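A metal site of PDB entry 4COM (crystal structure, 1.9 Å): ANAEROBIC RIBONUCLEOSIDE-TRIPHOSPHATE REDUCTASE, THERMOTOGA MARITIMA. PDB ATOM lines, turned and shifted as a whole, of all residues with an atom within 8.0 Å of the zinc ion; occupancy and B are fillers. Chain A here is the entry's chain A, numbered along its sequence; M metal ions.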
ATOM      1  N   GLU A 276       4.253  -9.649  36.067  1.00  0.00           N
ATOM      2  CA  GLU A 276       4.259  -9.455  34.614  1.00  0.00           C
ATOM      3  C   GLU A 276       3.755  -8.060  34.224  1.00  0.00           C
ATOM      4  O   GLU A 276       4.161  -7.488  33.195  1.00  0.00           O
ATOM      5  CB  GLU A 276       3.400 -10.510  33.912  1.00  0.00           C
ATOM      6  CG  GLU A 276       3.747 -11.959  34.257  1.00  0.00           C
ATOM      7  CD  GLU A 276       2.805 -12.971  33.607  1.00  0.00           C
ATOM      8  OE1 GLU A 276       2.034 -12.580  32.702  1.00  0.00           O
ATOM      9  OE2 GLU A 276       2.834 -14.152  33.996  1.00  0.00           O
ATOM     10  N   ARG A 277       2.844  -7.506  35.022  1.00  0.00           N
ATOM     11  CA  ARG A 277       2.283  -6.177  34.706  1.00  0.00           C
ATOM     12  C   ARG A 277       3.226  -5.063  35.227  1.00  0.00           C
ATOM     13  O   ARG A 277       3.295  -3.968  34.638  1.00  0.00           O
ATOM     14  CB  ARG A 277       0.930  -5.940  35.356  1.00  0.00           C
ATOM     15  CG  ARG A 277      -0.139  -7.037  35.257  1.00  0.00           C
ATOM     16  CD  ARG A 277      -0.485  -7.414  33.855  1.00  0.00           C
ATOM     17  NE  ARG A 277      -0.883  -6.270  33.032  1.00  0.00           N
ATOM     18  CZ  ARG A 277      -1.134  -6.390  31.725  1.00  0.00           C
ATOM     19  NH1 ARG A 277      -1.059  -7.577  31.144  1.00  0.00           N
ATOM     20  NH2 ARG A 277      -1.471  -5.317  31.005  1.00  0.00           N
ATOM     21  N   VAL A 593      13.886  -6.661  33.051  1.00  0.00           N
ATOM     22  CA  VAL A 593      12.835  -5.626  32.896  1.00  0.00           C
ATOM     23  C   VAL A 593      13.078  -4.665  31.713  1.00  0.00           C
ATOM     24  O   VAL A 593      14.228  -4.373  31.354  1.00  0.00           O
ATOM     25  CB  VAL A 593      12.601  -4.769  34.186  1.00  0.00           C
ATOM     26  CG1 VAL A 593      12.057  -5.590  35.328  1.00  0.00           C
ATOM     27  CG2 VAL A 593      13.872  -4.050  34.621  1.00  0.00           C
ATOM     28  N   CYS A 594      11.982  -4.191  31.093  1.00  0.00           N
ATOM     29  CA  CYS A 594      12.042  -3.196  30.026  1.00  0.00           C
ATOM     30  C   CYS A 594      11.915  -1.771  30.603  1.00  0.00           C
ATOM     31  O   CYS A 594      11.786  -1.607  31.812  1.00  0.00           O
ATOM     32  CB  CYS A 594      10.920  -3.443  29.010  1.00  0.00           C
ATOM     33  SG  CYS A 594       9.271  -3.037  29.659  1.00  0.00           S
ATOM     34  N   GLU A 595      11.923  -0.748  29.737  1.00  0.00           N
ATOM     35  CA  GLU A 595      11.892   0.640  30.244  1.00  0.00           C
ATOM     36  C   GLU A 595      10.537   0.991  30.890  1.00  0.00           C
ATOM     37  O   GLU A 595      10.472   1.862  31.747  1.00  0.00           O
ATOM     38  CB  GLU A 595      12.295   1.658  29.170  1.00  0.00           C
ATOM     39  CG  GLU A 595      11.280   1.904  28.065  1.00  0.00           C
ATOM     40  CD  GLU A 595      11.747   2.977  27.068  1.00  0.00           C
ATOM     41  OE1 GLU A 595      12.858   3.521  27.238  1.00  0.00           O
ATOM     42  OE2 GLU A 595      10.990   3.276  26.116  1.00  0.00           O
ATOM     43  N   ASP A 596       9.474   0.261  30.515  1.00  0.00           N
ATOM     44  CA  ASP A 596       8.155   0.465  31.117  1.00  0.00           C
ATOM     45  C   ASP A 596       7.805  -0.503  32.287  1.00  0.00           C
ATOM     46  O   ASP A 596       6.681  -0.493  32.797  1.00  0.00           O
ATOM     47  CB  ASP A 596       7.095   0.470  30.016  1.00  0.00           C
ATOM     48  CG  ASP A 596       7.342   1.586  28.985  1.00  0.00           C
ATOM     49  OD1 ASP A 596       7.912   2.644  29.359  1.00  0.00           O
ATOM     50  OD2 ASP A 596       6.962   1.394  27.814  1.00  0.00           O
ATOM     51  N   GLY A 597       8.776  -1.299  32.726  1.00  0.00           N
ATOM     52  CA  GLY A 597       8.679  -2.016  33.990  1.00  0.00           C
ATOM     53  C   GLY A 597       8.029  -3.397  33.990  1.00  0.00           C
ATOM     54  O   GLY A 597       7.744  -3.927  35.064  1.00  0.00           O
ATOM     55  N   HIS A 598       7.769  -3.975  32.800  1.00  0.00           N
ATOM     56  CA  HIS A 598       7.307  -5.369  32.683  1.00  0.00           C
ATOM     57  C   HIS A 598       8.459  -6.353  33.044  1.00  0.00           C
ATOM     58  O   HIS A 598       9.594  -6.118  32.614  1.00  0.00           O
ATOM     59  CB  HIS A 598       6.833  -5.658  31.238  1.00  0.00           C
ATOM     60  CG  HIS A 598       5.915  -4.610  30.670  1.00  0.00           C
ATOM     61  ND1 HIS A 598       6.144  -3.985  29.460  1.00  0.00           N
ATOM     62  CD2 HIS A 598       4.740  -4.095  31.133  1.00  0.00           C
ATOM     63  CE1 HIS A 598       5.177  -3.114  29.215  1.00  0.00           C
ATOM     64  NE2 HIS A 598       4.317  -3.172  30.212  1.00  0.00           N
ATOM     65  N   ALA A 599       8.171  -7.407  33.812  1.00  0.00           N
ATOM     66  CA  ALA A 599       9.158  -8.475  34.119  1.00  0.00           C
ATOM     67  C   ALA A 599       9.078  -9.718  33.197  1.00  0.00           C
ATOM     68  O   ALA A 599       7.983 -10.192  32.865  1.00  0.00           O
ATOM     69  CB  ALA A 599       9.034  -8.935  35.608  1.00  0.00           C
ATOM     70  N   PHE A 600      10.252 -10.228  32.808  1.00  0.00           N
ATOM     71  CA  PHE A 600      10.342 -11.389  31.921  1.00  0.00           C
ATOM     72  C   PHE A 600      11.737 -12.029  31.970  1.00  0.00           C
ATOM     73  O   PHE A 600      12.575 -11.634  32.790  1.00  0.00           O
ATOM     74  CB  PHE A 600       9.953 -10.978  30.471  1.00  0.00           C
ATOM     75  CG  PHE A 600      10.788  -9.854  29.907  1.00  0.00           C
ATOM     76  CD1 PHE A 600      10.489  -8.530  30.196  1.00  0.00           C
ATOM     77  CD2 PHE A 600      11.869 -10.119  29.086  1.00  0.00           C
ATOM     78  CE1 PHE A 600      11.257  -7.485  29.673  1.00  0.00           C
ATOM     79  CE2 PHE A 600      12.641  -9.079  28.575  1.00  0.00           C
ATOM     80  CZ  PHE A 600      12.336  -7.763  28.864  1.00  0.00           C
ATOM     81  N   ARG A 604      13.918  -9.667  25.051  1.00  0.00           N
ATOM     82  CA  ARG A 604      12.797  -8.940  24.455  1.00  0.00           C
ATOM     83  C   ARG A 604      11.524  -9.131  25.259  1.00  0.00           C
ATOM     84  O   ARG A 604      11.101 -10.264  25.536  1.00  0.00           O
ATOM     85  CB  ARG A 604      12.560  -9.419  23.017  1.00  0.00           C
ATOM     86  CG  ARG A 604      11.262  -8.905  22.379  1.00  0.00           C
ATOM     87  CD  ARG A 604      11.088  -9.405  20.943  1.00  0.00           C
ATOM     88  NE  ARG A 604      12.033  -8.781  20.010  1.00  0.00           N
ATOM     89  CZ  ARG A 604      13.165  -9.341  19.561  1.00  0.00           C
ATOM     90  NH1 ARG A 604      13.535 -10.563  19.960  1.00  0.00           N
ATOM     91  NH2 ARG A 604      13.945  -8.679  18.707  1.00  0.00           N
ATOM     92  N   CYS A 605      10.887  -8.014  25.611  1.00  0.00           N
ATOM     93  CA  CYS A 605       9.671  -8.037  26.434  1.00  0.00           C
ATOM     94  C   CYS A 605       8.499  -8.703  25.676  1.00  0.00           C
ATOM     95  O   CYS A 605       8.182  -8.310  24.559  1.00  0.00           O
ATOM     96  CB  CYS A 605       9.278  -6.622  26.861  1.00  0.00           C
ATOM     97  SG  CYS A 605       7.790  -6.518  27.897  1.00  0.00           S
ATOM     98  N   PRO A 606       7.848  -9.696  26.306  1.00  0.00           N
ATOM     99  CA  PRO A 606       6.714 -10.351  25.633  1.00  0.00           C
ATOM    100  C   PRO A 606       5.393  -9.553  25.674  1.00  0.00           C
ATOM    101  O   PRO A 606       4.412 -10.002  25.058  1.00  0.00           O
ATOM    102  CB  PRO A 606       6.571 -11.673  26.385  1.00  0.00           C
ATOM    103  CG  PRO A 606       7.076 -11.375  27.775  1.00  0.00           C
ATOM    104  CD  PRO A 606       8.170 -10.340  27.604  1.00  0.00           C
ATOM    105  N   VAL A 607       5.378  -8.413  26.376  1.00  0.00           N
ATOM    106  CA  VAL A 607       4.189  -7.569  26.475  1.00  0.00           C
ATOM    107  C   VAL A 607       4.185  -6.430  25.443  1.00  0.00           C
ATOM    108  O   VAL A 607       3.189  -6.246  24.744  1.00  0.00           O
ATOM    109  CB  VAL A 607       4.038  -6.977  27.899  1.00  0.00           C
ATOM    110  CG1 VAL A 607       2.860  -5.989  27.984  1.00  0.00           C
ATOM    111  CG2 VAL A 607       3.912  -8.094  28.928  1.00  0.00           C
ATOM    112  N   CYS A 608       5.293  -5.690  25.354  1.00  0.00           N
ATOM    113  CA  CYS A 608       5.409  -4.474  24.500  1.00  0.00           C
ATOM    114  C   CYS A 608       6.550  -4.520  23.471  1.00  0.00           C
ATOM    115  O   CYS A 608       6.668  -3.620  22.625  1.00  0.00           O
ATOM    116  CB  CYS A 608       5.602  -3.233  25.375  1.00  0.00           C
ATOM    117  SG  CYS A 608       7.264  -3.044  26.151  1.00  0.00           S
ATOM    118  N   GLY A 609       7.405  -5.538  23.549  1.00  0.00           N
ATOM    119  CA  GLY A 609       8.417  -5.765  22.520  1.00  0.00           C
ATOM    120  C   GLY A 609       9.716  -4.972  22.584  1.00  0.00           C
ATOM    121  O   GLY A 609      10.559  -5.129  21.703  1.00  0.00           O
ATOM    122  N   LYS A 610       9.888  -4.148  23.619  1.00  0.00           N
ATOM    123  CA  LYS A 610      11.128  -3.377  23.814  1.00  0.00           C
ATOM    124  C   LYS A 610      12.252  -4.221  24.435  1.00  0.00           C
ATOM    125  O   LYS A 610      11.980  -5.245  25.066  1.00  0.00           O
ATOM    126  CB  LYS A 610      10.868  -2.183  24.747  1.00  0.00           C
ATOM    127  CG  LYS A 610      10.002  -1.070  24.146  1.00  0.00           C
ATOM    128  CD  LYS A 610       9.621  -0.041  25.218  1.00  0.00           C
ATOM    129  CE  LYS A 610       8.700   1.035  24.645  1.00  0.00           C
ATOM    130  NZ  LYS A 610       8.656   2.264  25.517  1.00  0.00           N
ATOM    131  N   ALA A 611      13.491  -3.771  24.288  1.00  0.00           N
ATOM    132  CA  ALA A 611      14.642  -4.478  24.849  1.00  0.00           C
ATOM    133  C   ALA A 611      14.719  -4.369  26.386  1.00  0.00           C
ATOM    134  O   ALA A 611      14.164  -3.455  26.992  1.00  0.00           O
ATOM    135  CB  ALA A 611      15.922  -3.954  24.239  1.00  0.00           C
ATOM    136  N   LYS A 612      15.408  -5.317  27.016  1.00  0.00           N
ATOM    137  CA  LYS A 612      15.693  -5.211  28.441  1.00  0.00           C
ATOM    138  C   LYS A 612      16.681  -4.077  28.732  1.00  0.00           C
ATOM    139  O   LYS A 612      17.598  -3.810  27.929  1.00  0.00           O
ATOM    140  CB  LYS A 612      16.184  -6.543  29.011  1.00  0.00           C
ATOM    141  CG  LYS A 612      17.690  -6.762  29.045  1.00  0.00           C
ATOM    142  CD  LYS A 612      18.025  -7.879  30.034  1.00  0.00           C
ATOM    143  CE  LYS A 612      19.531  -8.087  30.183  1.00  0.00           C
ATOM    144  NZ  LYS A 612      19.851  -9.033  31.305  1.00  0.00           N
HETATM  145 ZN    ZN M   1       7.609  -4.197  28.218  1.00  0.00          ZN
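SG of Cys 605 lies close to N of Val 607.
The backbone carbonyl oxygen (O) of Lys 610 is in hydrogen-bond range of the backbone NH (N) of Cys 605 (3.0 Å).
The side-chain sulfur (SG) of Cys 594 sits close to the backbone NH (N) of Asp 596 (3.4 Å).
The backbone NH (N) of Gly 597 lies close to the side-chain sulfur (SG) of Cys 594, 3.6 Å away.
Within 4 Å of the zinc ion: Cys 594, His 598, Cys 605 and Cys 608.
The nearest printed residue that does not touch the zinc ion is Val 607 (4.5 Å).
The zinc ion is bound by ND1 of His 598 (1.9 Å), SG of Cys 605 (2.4 Å), SG of Cys 608 (2.4 Å) and SG of Cys 594 (2.5 Å).
The zinc ion has four donor atoms within binding distance.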
